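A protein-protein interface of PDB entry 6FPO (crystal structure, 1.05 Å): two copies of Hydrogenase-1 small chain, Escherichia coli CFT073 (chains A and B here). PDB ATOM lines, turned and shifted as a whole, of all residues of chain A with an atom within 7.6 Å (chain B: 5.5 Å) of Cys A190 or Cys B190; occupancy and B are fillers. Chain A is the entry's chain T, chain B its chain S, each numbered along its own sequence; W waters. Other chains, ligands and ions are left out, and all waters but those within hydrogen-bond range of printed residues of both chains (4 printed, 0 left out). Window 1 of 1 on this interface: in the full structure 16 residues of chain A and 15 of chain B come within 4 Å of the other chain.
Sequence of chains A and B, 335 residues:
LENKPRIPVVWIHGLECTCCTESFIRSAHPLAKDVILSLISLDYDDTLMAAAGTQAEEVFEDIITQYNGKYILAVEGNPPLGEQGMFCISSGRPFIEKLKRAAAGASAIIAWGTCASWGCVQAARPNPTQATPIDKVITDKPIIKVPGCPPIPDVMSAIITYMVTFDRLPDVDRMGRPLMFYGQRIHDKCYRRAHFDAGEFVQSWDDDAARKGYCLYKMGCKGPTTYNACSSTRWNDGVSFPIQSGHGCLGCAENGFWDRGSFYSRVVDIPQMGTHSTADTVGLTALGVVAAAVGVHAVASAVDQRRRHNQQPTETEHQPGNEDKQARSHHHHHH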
ATOM      1  N   ARG A 185     -22.086 -16.877  24.724  1.00  0.00           N
ATOM      2  CA  ARG A 185     -22.066 -15.868  25.821  1.00  0.00           C
ATOM      3  C   ARG A 185     -23.403 -15.117  26.071  1.00  0.00           C
ATOM      4  O   ARG A 185     -24.236 -14.921  25.140  1.00  0.00           O
ATOM      5  CB  ARG A 185     -21.001 -14.795  25.540  1.00  0.00           C
ATOM      6  CG  ARG A 185     -19.610 -15.345  25.320  1.00  0.00           C
ATOM      7  CD  ARG A 185     -18.663 -14.190  24.903  1.00  0.00           C
ATOM      8  NE  ARG A 185     -17.348 -14.579  24.492  1.00  0.00           N
ATOM      9  CZ  ARG A 185     -17.000 -14.819  23.238  1.00  0.00           C
ATOM     10  NH1 ARG A 185     -17.886 -14.721  22.260  1.00  0.00           N
ATOM     11  NH2 ARG A 185     -15.763 -15.179  22.970  1.00  0.00           N
ATOM     12  N   ILE A 186     -23.605 -14.687  27.269  1.00  0.00           N
ATOM     13  CA  ILE A 186     -24.757 -13.854  27.577  1.00  0.00           C
ATOM     14  C   ILE A 186     -24.838 -12.670  26.595  1.00  0.00           C
ATOM     15  O   ILE A 186     -25.903 -12.350  26.041  1.00  0.00           O
ATOM     16  CB  ILE A 186     -24.649 -13.321  29.047  1.00  0.00           C
ATOM     17  CG1 ILE A 186     -24.788 -14.496  30.052  1.00  0.00           C
ATOM     18  CG2 ILE A 186     -25.633 -12.217  29.349  1.00  0.00           C
ATOM     19  CD1 ILE A 186     -26.097 -15.157  30.040  1.00  0.00           C
ATOM     20  N   HIS A 187     -23.715 -12.006  26.398  1.00  0.00           N
ATOM     21  CA  HIS A 187     -23.600 -10.811  25.579  1.00  0.00           C
ATOM     22  C   HIS A 187     -23.841 -11.082  24.099  1.00  0.00           C
ATOM     23  O   HIS A 187     -24.043 -10.132  23.360  1.00  0.00           O
ATOM     24  CB  HIS A 187     -22.212 -10.223  25.871  1.00  0.00           C
ATOM     25  CG  HIS A 187     -21.754  -9.005  25.146  1.00  0.00           C
ATOM     26  ND1 HIS A 187     -22.159  -7.712  25.466  1.00  0.00           N
ATOM     27  CD2 HIS A 187     -20.730  -8.878  24.269  1.00  0.00           C
ATOM     28  CE1 HIS A 187     -21.448  -6.870  24.739  1.00  0.00           C
ATOM     29  NE2 HIS A 187     -20.574  -7.555  24.005  1.00  0.00           N
ATOM     30  N   ASP A 188     -23.729 -12.333  23.639  1.00  0.00           N
ATOM     31  CA  ASP A 188     -23.975 -12.557  22.248  1.00  0.00           C
ATOM     32  C   ASP A 188     -25.442 -12.870  21.940  1.00  0.00           C
ATOM     33  O   ASP A 188     -25.798 -13.080  20.803  1.00  0.00           O
ATOM     34  CB  ASP A 188     -23.017 -13.593  21.689  1.00  0.00           C
ATOM     35  CG  ASP A 188     -21.555 -13.119  21.693  1.00  0.00           C
ATOM     36  OD1 ASP A 188     -21.328 -11.901  21.591  1.00  0.00           O
ATOM     37  OD2 ASP A 188     -20.645 -13.964  21.787  1.00  0.00           O
ATOM     38  N   LYS A 189     -26.290 -12.887  22.994  1.00  0.00           N
ATOM     39  CA  LYS A 189     -27.722 -13.004  22.846  1.00  0.00           C
ATOM     40  C   LYS A 189     -28.464 -11.981  23.709  1.00  0.00           C
ATOM     41  O   LYS A 189     -29.595 -12.186  24.116  1.00  0.00           O
ATOM     42  CB  LYS A 189     -28.215 -14.437  23.142  1.00  0.00           C
ATOM     43  CG  LYS A 189     -27.952 -15.420  21.988  1.00  0.00           C
ATOM     44  CD  LYS A 189     -28.677 -15.023  20.713  1.00  0.00           C
ATOM     45  CE  LYS A 189     -28.955 -16.211  19.771  1.00  0.00           C
ATOM     46  NZ  LYS A 189     -27.713 -16.816  19.243  1.00  0.00           N
ATOM     47  N   CYS A 190     -27.811 -10.871  24.040  1.00  0.00           N
ATOM     48  CA  CYS A 190     -28.397  -9.893  24.925  1.00  0.00           C
ATOM     49  C   CYS A 190     -29.217  -8.864  24.170  1.00  0.00           C
ATOM     50  O   CYS A 190     -28.723  -8.211  23.246  1.00  0.00           O
ATOM     51  CB  CYS A 190     -27.296  -9.162  25.737  1.00  0.00           C
ATOM     52  SG  CYS A 190     -28.013  -7.981  26.949  1.00  0.00           S
ATOM     53  N   TYR A 191     -30.463  -8.662  24.619  1.00  0.00           N
ATOM     54  CA  TYR A 191     -31.366  -7.706  23.988  1.00  0.00           C
ATOM     55  C   TYR A 191     -30.930  -6.263  24.141  1.00  0.00           C
ATOM     56  O   TYR A 191     -31.511  -5.408  23.468  1.00  0.00           O
ATOM     57  CB  TYR A 191     -32.811  -7.930  24.440  1.00  0.00           C
ATOM     58  CG  TYR A 191     -33.188  -7.283  25.762  1.00  0.00           C
ATOM     59  CD1 TYR A 191     -32.487  -7.471  26.943  1.00  0.00           C
ATOM     60  CD2 TYR A 191     -34.287  -6.474  25.812  1.00  0.00           C
ATOM     61  CE1 TYR A 191     -32.854  -6.827  28.102  1.00  0.00           C
ATOM     62  CE2 TYR A 191     -34.680  -5.817  26.955  1.00  0.00           C
ATOM     63  CZ  TYR A 191     -33.945  -5.988  28.121  1.00  0.00           C
ATOM     64  OH  TYR A 191     -34.234  -5.307  29.288  1.00  0.00           O
ATOM     65  N   ARG A 192     -29.936  -5.944  24.978  1.00  0.00           N
ATOM     66  CA  ARG A 192     -29.417  -4.586  25.063  1.00  0.00           C
ATOM     67  C   ARG A 192     -28.192  -4.373  24.208  1.00  0.00           C
ATOM     68  O   ARG A 192     -27.568  -3.288  24.266  1.00  0.00           O
ATOM     69  CB  ARG A 192     -29.143  -4.166  26.533  1.00  0.00           C
ATOM     70  CG  ARG A 192     -30.384  -4.223  27.377  1.00  0.00           C
ATOM     71  CD  ARG A 192     -30.189  -3.663  28.761  1.00  0.00           C
ATOM     72  NE  ARG A 192     -31.427  -3.812  29.548  1.00  0.00           N
ATOM     73  CZ  ARG A 192     -31.725  -3.108  30.629  1.00  0.00           C
ATOM     74  NH1 ARG A 192     -30.931  -2.159  31.088  1.00  0.00           N
ATOM     75  NH2 ARG A 192     -32.873  -3.354  31.235  1.00  0.00           N
ATOM     76  N   ARG A 193     -27.825  -5.337  23.377  1.00  0.00           N
ATOM     77  CA  ARG A 193     -26.620  -5.211  22.582  1.00  0.00           C
ATOM     78  C   ARG A 193     -26.690  -4.018  21.595  1.00  0.00           C
ATOM     79  O   ARG A 193     -25.658  -3.386  21.326  1.00  0.00           O
ATOM     80  CB  ARG A 193     -26.353  -6.541  21.910  1.00  0.00           C
ATOM     81  CG  ARG A 193     -25.082  -6.598  21.116  1.00  0.00           C
ATOM     82  CD  ARG A 193     -23.777  -6.449  21.929  1.00  0.00           C
ATOM     83  NE  ARG A 193     -22.649  -6.529  21.016  1.00  0.00           N
ATOM     84  CZ  ARG A 193     -22.017  -7.648  20.689  1.00  0.00           C
ATOM     85  NH1 ARG A 193     -22.302  -8.798  21.254  1.00  0.00           N
ATOM     86  NH2 ARG A 193     -21.084  -7.601  19.776  1.00  0.00           N
ATOM     87  N   ALA A 194     -27.896  -3.680  21.106  1.00  0.00           N
ATOM     88  CA  ALA A 194     -27.990  -2.503  20.237  1.00  0.00           C
ATOM     89  C   ALA A 194     -27.410  -1.283  20.922  1.00  0.00           C
ATOM     90  O   ALA A 194     -26.780  -0.422  20.310  1.00  0.00           O
ATOM     91  CB  ALA A 194     -29.415  -2.211  19.895  1.00  0.00           C
ATOM     92  N   HIS A 195     -27.699  -1.164  22.213  1.00  0.00           N
ATOM     93  CA  HIS A 195     -27.213  -0.024  22.993  1.00  0.00           C
ATOM     94  C   HIS A 195     -25.714  -0.080  23.185  1.00  0.00           C
ATOM     95  O   HIS A 195     -25.005   0.915  23.030  1.00  0.00           O
ATOM     96  CB  HIS A 195     -27.945   0.068  24.307  1.00  0.00           C
ATOM     97  CG  HIS A 195     -29.425   0.227  24.157  1.00  0.00           C
ATOM     98  ND1 HIS A 195     -29.989   1.247  23.412  1.00  0.00           N
ATOM     99  CD2 HIS A 195     -30.455  -0.507  24.616  1.00  0.00           C
ATOM    100  CE1 HIS A 195     -31.314   1.096  23.460  1.00  0.00           C
ATOM    101  NE2 HIS A 195     -31.622   0.059  24.207  1.00  0.00           N
ATOM    102  N   PHE A 196     -25.201  -1.256  23.505  1.00  0.00           N
ATOM    103  CA  PHE A 196     -23.724  -1.431  23.570  1.00  0.00           C
ATOM    104  C   PHE A 196     -23.085  -0.978  22.294  1.00  0.00           C
ATOM    105  O   PHE A 196     -22.101  -0.192  22.303  1.00  0.00           O
ATOM    106  CB  PHE A 196     -23.385  -2.899  23.824  1.00  0.00           C
ATOM    107  CG  PHE A 196     -21.927  -3.212  23.919  1.00  0.00           C
ATOM    108  CD1 PHE A 196     -21.242  -3.148  25.124  1.00  0.00           C
ATOM    109  CD2 PHE A 196     -21.224  -3.601  22.782  1.00  0.00           C
ATOM    110  CE1 PHE A 196     -19.901  -3.442  25.204  1.00  0.00           C
ATOM    111  CE2 PHE A 196     -19.865  -3.924  22.875  1.00  0.00           C
ATOM    112  CZ  PHE A 196     -19.215  -3.844  24.096  1.00  0.00           C
ATOM    113  N   CYS A 215     -27.539  -0.255  27.856  1.00  0.00           N
ATOM    114  CA  CYS A 215     -26.572  -1.294  28.238  1.00  0.00           C
ATOM    115  C   CYS A 215     -25.926  -0.982  29.571  1.00  0.00           C
ATOM    116  O   CYS A 215     -25.667   0.173  29.935  1.00  0.00           O
ATOM    117  CB  CYS A 215     -25.523  -1.390  27.093  1.00  0.00           C
ATOM    118  SG  CYS A 215     -24.065  -2.410  27.474  1.00  0.00           S
ATOM    119  N   LEU A 216     -25.628  -2.076  30.295  1.00  0.00           N
ATOM    120  CA  LEU A 216     -25.080  -2.067  31.671  1.00  0.00           C
ATOM    121  C   LEU A 216     -23.582  -2.267  31.714  1.00  0.00           C
ATOM    122  O   LEU A 216     -23.018  -2.417  32.831  1.00  0.00           O
ATOM    123  CB  LEU A 216     -25.832  -3.088  32.492  1.00  0.00           C
ATOM    124  CG  LEU A 216     -27.329  -2.818  32.592  1.00  0.00           C
ATOM    125  CD1 LEU A 216     -28.076  -3.965  33.218  1.00  0.00           C
ATOM    126  CD2 LEU A 216     -27.650  -1.537  33.266  1.00  0.00           C
ATOM    127  N   CYS A 221     -21.379  -4.875  34.018  1.00  0.00           N
ATOM    128  CA  CYS A 221     -21.914  -6.152  33.450  1.00  0.00           C
ATOM    129  C   CYS A 221     -20.805  -7.053  32.948  1.00  0.00           C
ATOM    130  O   CYS A 221     -19.977  -6.625  32.123  1.00  0.00           O
ATOM    131  CB  CYS A 221     -22.831  -5.766  32.299  1.00  0.00           C
ATOM    132  SG  CYS A 221     -23.672  -7.254  31.629  1.00  0.00           S
ATOM    133  N   GLY A 223     -21.526  -9.847  31.270  1.00  0.00           N
ATOM    134  CA  GLY A 223     -22.047 -10.626  30.159  1.00  0.00           C
ATOM    135  C   GLY A 223     -21.053 -10.939  29.045  1.00  0.00           C
ATOM    136  O   GLY A 223     -21.111 -12.029  28.470  1.00  0.00           O
ATOM    137  N   CYS A 230     -29.029 -17.149  30.006  1.00  0.00           N
ATOM    138  CA  CYS A 230     -29.947 -16.237  30.691  1.00  0.00           C
ATOM    139  C   CYS A 230     -30.593 -15.233  29.768  1.00  0.00           C
ATOM    140  O   CYS A 230     -31.705 -14.796  30.033  1.00  0.00           O
ATOM    141  CB  CYS A 230     -29.195 -15.495  31.800  1.00  0.00           C
ATOM    142  SG  CYS A 230     -28.300 -16.648  32.861  1.00  0.00           S
ATOM    143  N   SER A 231     -29.886 -14.796  28.721  1.00  0.00           N
ATOM    144  CA  SER A 231     -30.392 -13.781  27.813  1.00  0.00           C
ATOM    145  C   SER A 231     -31.313 -14.328  26.729  1.00  0.00           C
ATOM    146  O   SER A 231     -31.880 -13.552  25.976  1.00  0.00           O
ATOM    147  CB  SER A 231     -29.245 -12.970  27.237  1.00  0.00           C
ATOM    148  OG  SER A 231     -28.270 -13.851  26.691  1.00  0.00           O
ATOM    149  N   SER A 232     -31.487 -15.640  26.682  1.00  0.00           N
ATOM    150  CA  SER A 232     -32.280 -16.338  25.643  1.00  0.00           C
ATOM    151  C   SER A 232     -33.412 -17.113  26.309  1.00  0.00           C
ATOM    152  O   SER A 232     -34.607 -16.810  26.167  1.00  0.00           O
ATOM    153  CB  SER A 232     -31.400 -17.331  24.838  1.00  0.00           C
ATOM    154  OG  SER A 232     -30.489 -16.698  23.987  1.00  0.00           O
ATOM    155  N   PHE A 241     -34.370 -11.737  33.443  1.00  0.00           N
ATOM    156  CA  PHE A 241     -33.017 -12.173  33.777  1.00  0.00           C
ATOM    157  C   PHE A 241     -32.326 -10.957  34.401  1.00  0.00           C
ATOM    158  O   PHE A 241     -32.856  -9.859  34.346  1.00  0.00           O
ATOM    159  CB  PHE A 241     -32.258 -12.839  32.573  1.00  0.00           C
ATOM    160  CG  PHE A 241     -31.714 -11.926  31.533  1.00  0.00           C
ATOM    161  CD1 PHE A 241     -32.573 -11.274  30.639  1.00  0.00           C
ATOM    162  CD2 PHE A 241     -30.350 -11.803  31.307  1.00  0.00           C
ATOM    163  CE1 PHE A 241     -32.053 -10.500  29.588  1.00  0.00           C
ATOM    164  CE2 PHE A 241     -29.856 -11.073  30.263  1.00  0.00           C
ATOM    165  CZ  PHE A 241     -30.707 -10.425  29.415  1.00  0.00           C
ATOM    166  N   ILE A 243     -30.006  -8.726  33.681  1.00  0.00           N
ATOM    167  CA  ILE A 243     -29.863  -7.518  32.876  1.00  0.00           C
ATOM    168  C   ILE A 243     -31.232  -6.901  32.566  1.00  0.00           C
ATOM    169  O   ILE A 243     -31.398  -5.688  32.574  1.00  0.00           O
ATOM    170  CB  ILE A 243     -29.075  -7.863  31.625  1.00  0.00           C
ATOM    171  CG1 ILE A 243     -27.591  -8.052  31.971  1.00  0.00           C
ATOM    172  CG2 ILE A 243     -29.239  -6.811  30.528  1.00  0.00           C
ATOM    173  CD1 ILE A 243     -26.890  -9.072  31.103  1.00  0.00           C
ATOM    174  N   GLN A 244     -32.230  -7.735  32.262  1.00  0.00           N
ATOM    175  CA  GLN A 244     -33.558  -7.214  31.954  1.00  0.00           C
ATOM    176  C   GLN A 244     -34.133  -6.413  33.090  1.00  0.00           C
ATOM    177  O   GLN A 244     -34.854  -5.449  32.844  1.00  0.00           O
ATOM    178  CB  GLN A 244     -34.457  -8.378  31.527  1.00  0.00           C
ATOM    179  CG  GLN A 244     -35.791  -7.967  31.012  1.00  0.00           C
ATOM    180  CD  GLN A 244     -36.554  -9.160  30.495  1.00  0.00           C
ATOM    181  OE1 GLN A 244     -36.021  -9.934  29.616  1.00  0.00           O
ATOM    182  NE2 GLN A 244     -37.766  -9.278  30.930  1.00  0.00           N
ATOM    183  N   ILE B 186     -37.872  -2.534  17.134  1.00  0.00           N
ATOM    184  CA  ILE B 186     -37.623  -3.942  17.404  1.00  0.00           C
ATOM    185  C   ILE B 186     -36.133  -4.210  17.462  1.00  0.00           C
ATOM    186  O   ILE B 186     -35.619  -4.888  18.373  1.00  0.00           O
ATOM    187  CB  ILE B 186     -38.315  -4.821  16.300  1.00  0.00           C
ATOM    188  CG1 ILE B 186     -39.840  -4.724  16.392  1.00  0.00           C
ATOM    189  CG2 ILE B 186     -37.816  -6.270  16.324  1.00  0.00           C
ATOM    190  CD1 ILE B 186     -40.429  -5.293  17.589  1.00  0.00           C
ATOM    191  N   HIS B 187     -35.284  -4.116  16.528  1.00  0.00           N
ATOM    192  CA  HIS B 187     -33.861  -4.040  16.192  1.00  0.00           C
ATOM    193  C   HIS B 187     -32.993  -3.324  17.225  1.00  0.00           C
ATOM    194  O   HIS B 187     -31.777  -3.510  17.254  1.00  0.00           O
ATOM    195  CB  HIS B 187     -33.676  -3.388  14.819  1.00  0.00           C
ATOM    196  CG  HIS B 187     -32.262  -3.412  14.326  1.00  0.00           C
ATOM    197  ND1 HIS B 187     -31.610  -4.578  13.989  1.00  0.00           N
ATOM    198  CD2 HIS B 187     -31.375  -2.410  14.112  1.00  0.00           C
ATOM    199  CE1 HIS B 187     -30.384  -4.296  13.589  1.00  0.00           C
ATOM    200  NE2 HIS B 187     -30.215  -2.986  13.654  1.00  0.00           N
ATOM    201  N   ASP B 188     -33.641  -2.301  18.115  1.00  0.00           N
ATOM    202  CA  ASP B 188     -32.844  -1.700  19.163  1.00  0.00           C
ATOM    203  C   ASP B 188     -33.015  -2.429  20.510  1.00  0.00           C
ATOM    204  O   ASP B 188     -32.384  -2.028  21.472  1.00  0.00           O
ATOM    205  CB  ASP B 188     -33.118  -0.201  19.252  1.00  0.00           C
ATOM    206  CG  ASP B 188     -32.619   0.573  18.038  1.00  0.00           C
ATOM    207  OD1 ASP B 188     -31.689   0.101  17.345  1.00  0.00           O
ATOM    208  OD2 ASP B 188     -33.204   1.631  17.706  1.00  0.00           O
ATOM    209  N   LYS B 189     -33.861  -3.483  20.539  1.00  0.00           N
ATOM    210  CA  LYS B 189     -34.001  -4.359  21.693  1.00  0.00           C
ATOM    211  C   LYS B 189     -33.992  -5.825  21.285  1.00  0.00           C
ATOM    212  O   LYS B 189     -34.524  -6.694  21.977  1.00  0.00           O
ATOM    213  CB  LYS B 189     -35.226  -4.023  22.525  1.00  0.00           C
ATOM    214  CG  LYS B 189     -35.079  -2.783  23.395  1.00  0.00           C
ATOM    215  CD  LYS B 189     -33.976  -2.918  24.432  1.00  0.00           C
ATOM    216  CE  LYS B 189     -34.141  -2.053  25.646  1.00  0.00           C
ATOM    217  NZ  LYS B 189     -34.071  -0.602  25.315  1.00  0.00           N
ATOM    218  N   CYS B 190     -33.337  -6.141  20.155  1.00  0.00           N
ATOM    219  CA  CYS B 190     -33.349  -7.511  19.642  1.00  0.00           C
ATOM    220  C   CYS B 190     -32.175  -8.310  20.168  1.00  0.00           C
ATOM    221  O   CYS B 190     -31.013  -7.914  20.031  1.00  0.00           O
ATOM    222  CB  CYS B 190     -33.327  -7.494  18.096  1.00  0.00           C
ATOM    223  SG  CYS B 190     -33.408  -9.199  17.402  1.00  0.00           S
ATOM    224  N   TYR B 191     -32.479  -9.486  20.696  1.00  0.00           N
ATOM    225  CA  TYR B 191     -31.426 -10.365  21.244  1.00  0.00           C
ATOM    226  C   TYR B 191     -30.506 -10.953  20.203  1.00  0.00           C
ATOM    227  O   TYR B 191     -29.489 -11.515  20.602  1.00  0.00           O
ATOM    228  CB  TYR B 191     -32.065 -11.463  22.133  1.00  0.00           C
ATOM    229  CG  TYR B 191     -32.583 -12.668  21.399  1.00  0.00           C
ATOM    230  CD1 TYR B 191     -33.490 -12.603  20.332  1.00  0.00           C
ATOM    231  CD2 TYR B 191     -32.159 -13.934  21.773  1.00  0.00           C
ATOM    232  CE1 TYR B 191     -33.923 -13.745  19.679  1.00  0.00           C
ATOM    233  CE2 TYR B 191     -32.580 -15.079  21.124  1.00  0.00           C
ATOM    234  CZ  TYR B 191     -33.448 -14.974  20.042  1.00  0.00           C
ATOM    235  OH  TYR B 191     -33.824 -16.079  19.314  1.00  0.00           O
ATOM    236  N   ARG B 192     -30.777 -10.785  18.903  1.00  0.00           N
ATOM    237  CA  ARG B 192     -29.843 -11.210  17.871  1.00  0.00           C
ATOM    238  C   ARG B 192     -28.944 -10.087  17.378  1.00  0.00           C
ATOM    239  O   ARG B 192     -28.155 -10.296  16.434  1.00  0.00           O
ATOM    240  CB  ARG B 192     -30.562 -11.917  16.700  1.00  0.00           C
ATOM    241  CG  ARG B 192     -31.320 -13.148  17.155  1.00  0.00           C
ATOM    242  CD  ARG B 192     -31.913 -13.950  16.018  1.00  0.00           C
ATOM    243  NE  ARG B 192     -32.685 -15.069  16.504  1.00  0.00           N
ATOM    244  CZ  ARG B 192     -32.968 -16.167  15.815  1.00  0.00           C
ATOM    245  NH1 ARG B 192     -32.541 -16.327  14.582  1.00  0.00           N
ATOM    246  NH2 ARG B 192     -33.714 -17.094  16.410  1.00  0.00           N
ATOM    247  N   ARG B 193     -29.016  -8.920  18.022  1.00  0.00           N
ATOM    248  CA  ARG B 193     -28.236  -7.805  17.533  1.00  0.00           C
ATOM    249  C   ARG B 193     -26.716  -8.064  17.594  1.00  0.00           C
ATOM    250  O   ARG B 193     -26.003  -7.551  16.749  1.00  0.00           O
ATOM    251  CB  ARG B 193     -28.680  -6.573  18.309  1.00  0.00           C
ATOM    252  CG  ARG B 193     -28.043  -5.284  17.872  1.00  0.00           C
ATOM    253  CD  ARG B 193     -28.394  -4.843  16.459  1.00  0.00           C
ATOM    254  NE  ARG B 193     -27.719  -3.586  16.206  1.00  0.00           N
ATOM    255  CZ  ARG B 193     -28.240  -2.369  16.404  1.00  0.00           C
ATOM    256  NH1 ARG B 193     -29.490  -2.154  16.818  1.00  0.00           N
ATOM    257  NH2 ARG B 193     -27.468  -1.318  16.169  1.00  0.00           N
ATOM    258  N   ALA B 194     -26.240  -8.852  18.551  1.00  0.00           N
ATOM    259  CA  ALA B 194     -24.824  -9.199  18.554  1.00  0.00           C
ATOM    260  C   ALA B 194     -24.404  -9.778  17.231  1.00  0.00           C
ATOM    261  O   ALA B 194     -23.282  -9.550  16.715  1.00  0.00           O
ATOM    262  CB  ALA B 194     -24.524 -10.237  19.643  1.00  0.00           C
ATOM    263  N   SER B 231     -39.627  -7.536  20.820  1.00  0.00           N
ATOM    264  CA  SER B 231     -38.325  -8.066  21.213  1.00  0.00           C
ATOM    265  C   SER B 231     -38.034  -7.926  22.712  1.00  0.00           C
ATOM    266  O   SER B 231     -36.992  -8.409  23.178  1.00  0.00           O
ATOM    267  CB  SER B 231     -37.236  -7.448  20.358  1.00  0.00           C
ATOM    268  OG  SER B 231     -37.347  -6.020  20.353  1.00  0.00           O
ATOM    269  N   PHE B 241     -41.287 -14.500  20.023  1.00  0.00           N
ATOM    270  CA  PHE B 241     -41.702 -13.452  19.101  1.00  0.00           C
ATOM    271  C   PHE B 241     -41.217 -13.899  17.725  1.00  0.00           C
ATOM    272  O   PHE B 241     -40.468 -14.877  17.613  1.00  0.00           O
ATOM    273  CB  PHE B 241     -41.218 -12.036  19.505  1.00  0.00           C
ATOM    274  CG  PHE B 241     -39.779 -11.699  19.301  1.00  0.00           C
ATOM    275  CD1 PHE B 241     -38.795 -12.252  20.068  1.00  0.00           C
ATOM    276  CD2 PHE B 241     -39.426 -10.688  18.402  1.00  0.00           C
ATOM    277  CE1 PHE B 241     -37.469 -11.821  19.936  1.00  0.00           C
ATOM    278  CE2 PHE B 241     -38.126 -10.268  18.284  1.00  0.00           C
ATOM    279  CZ  PHE B 241     -37.140 -10.851  19.080  1.00  0.00           C
ATOM    280  N   ILE B 243     -38.906 -13.224  15.468  1.00  0.00           N
ATOM    281  CA  ILE B 243     -37.485 -13.436  15.255  1.00  0.00           C
ATOM    282  C   ILE B 243     -36.980 -14.589  16.108  1.00  0.00           C
ATOM    283  O   ILE B 243     -36.149 -15.377  15.683  1.00  0.00           O
ATOM    284  CB  ILE B 243     -36.748 -12.125  15.542  1.00  0.00           C
ATOM    285  CG1 ILE B 243     -36.983 -11.123  14.407  1.00  0.00           C
ATOM    286  CG2 ILE B 243     -35.245 -12.312  15.784  1.00  0.00           C
ATOM    287  CD1 ILE B 243     -36.995  -9.685  14.841  1.00  0.00           C
HETATM  288  O   HOH W   1     -27.530  -9.570  21.016  1.00  0.00           O
HETATM  289  O   HOH W   2     -21.060  -9.632  18.451  1.00  0.00           O
HETATM  290  O   HOH W   3     -30.253  -5.276  20.989  1.00  0.00           O
HETATM  291  O   HOH W   4     -27.445   0.488  17.752  1.00  0.00           O
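Among the printed residues, pairs that only touch across the chains: His A187 with Ala B194 (3.7 Å), Asp A188 with Ala B194 (3.3 Å), Lys A189 with Tyr B191 (3.2 Å), Cys A190 with Cys B190 (3.96 Å), Cys A190 with Tyr B191 (3.9 Å), Tyr A191 with Lys B189 (3.2 Å), Tyr A191 with Cys B190 (3.9 Å), Tyr A191 with Tyr B191 (3.8 Å), Arg A193 with Ala B194 (3.1 Å), Ala A194 with His B187 (3.8 Å), Ala A194 with Asp B188 (3.4 Å), Ala A194 with Arg B193 (3.1 Å), His A195 with Asp B188 (3.5 Å) and Ser A232 with Tyr B191 (3.9 Å).
Water W4 bridges NH2 of Arg B193 (2.4 Å) and O of Ala A194 (2.8 Å).
Water W2 bridges NH2 of Arg A193 and O of Ala B194.
Water W3 lies within hydrogen-bond range of O of Tyr A191 (2.8 Å), N of Ala A194 (2.8 Å), O of Cys B190 (2.9 Å) and N of Arg A193 (3.4 Å).
Water W1 lies within hydrogen-bond range of the backbone carbonyl oxygen of Tyr B191, the backbone carbonyl oxygen of Cys A190, the backbone NH of Ala B194 and the backbone NH of Arg B193.
The side-chain hydroxyl (OH) of Tyr A191 lies within hydrogen-bond range of the guanidinium group (NH2) of Arg A192, at 3.1 Å.
OD1 of Asp A188 is in salt-bridge range of NH1 of Arg A193 (3.3 Å).
The guanidinium group (NH1) of Arg B193 lies within salt-bridge range of the side-chain carboxylate (OD1) of Asp B188 (3.2 Å).
The guanidinium group (NH1) of Arg A185 lies within salt-bridge range of the side-chain carboxylate (OD2) of Asp A188 (2.9 Å).
The side-chain sulfur (SG) of Cys A190 lies close to the backbone NH (N) of Arg A192 (3.4 Å).
The backbone carbonyl oxygen (O) of Lys A189 sits close to the side-chain hydroxyl (OG) of Ser A231, 3.3 Å away.
Lys A189 touches Tyr B191, and with the chains exchanged Tyr A191 touches Lys B189.
Cys A190 touches Tyr B191, and with the chains exchanged Tyr A191 touches Cys B190.
Tyr B191 touches its own counterpart, Tyr A191.
Arg A193 touches Ala B194, and with the chains exchanged Ala A194 touches Arg B193.
Positions printed for both chains: 186, 187, 188, 189, 190, 191, 192, 193, 194, 231, 241 and 243.
Of the 15 pairs that touch across the chains among the printed residues, 12 have their exchanged pair printed and touching as well.
Of the 12 printed residues of chain B, 7 touch a printed residue of chain A.
Hydrophobic or aromatic side chains of chain B within 4 Å of the printed part of chain A: Tyr B191 and Ala B194.
Hydrophobic or aromatic side chains of chain A within 4 Å of the printed part of chain B: Tyr A191, Ala A194 and His A195.
Among the printed residues, no Asp or Glu carboxylate lies within 4 Å of a Lys or Arg side-chain nitrogen of the other chain.
A ring nitrogen (NE2) of His A195 sits at hydrogen-bond distance from the side-chain amino group (NZ) of Lys B189 (2.8 Å).
Of the printed residues of chain B, Lys A189 touches Tyr B191 (3.2 Å).
Of chain B, only Cys B190 (3.96 Å) and Tyr B191 (3.9 Å) come within 4 Å of Cys A190.
Cys A230 touches none of the printed residues of chain B.
Ile B186 touches none of the printed residues of chain A.
Printed residues of chain A within 4 Å of Lys B189: Tyr A191 and His A195.
Of the printed residues of chain A, Cys B190 touches Cys A190 (3.96 Å) and Tyr A191 (3.9 Å).
Of the printed residues of chain A, Ala B194 touches His A187 (3.7 Å), Asp A188 (3.3 Å) and Arg A193 (3.1 Å).
The nearest printed residue of chain B that does not touch Cys A190 is Arg B193 (5.2 Å).
The nearest printed residue of chain A that does not touch Cys B190 is Arg A193 (5.2 Å).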
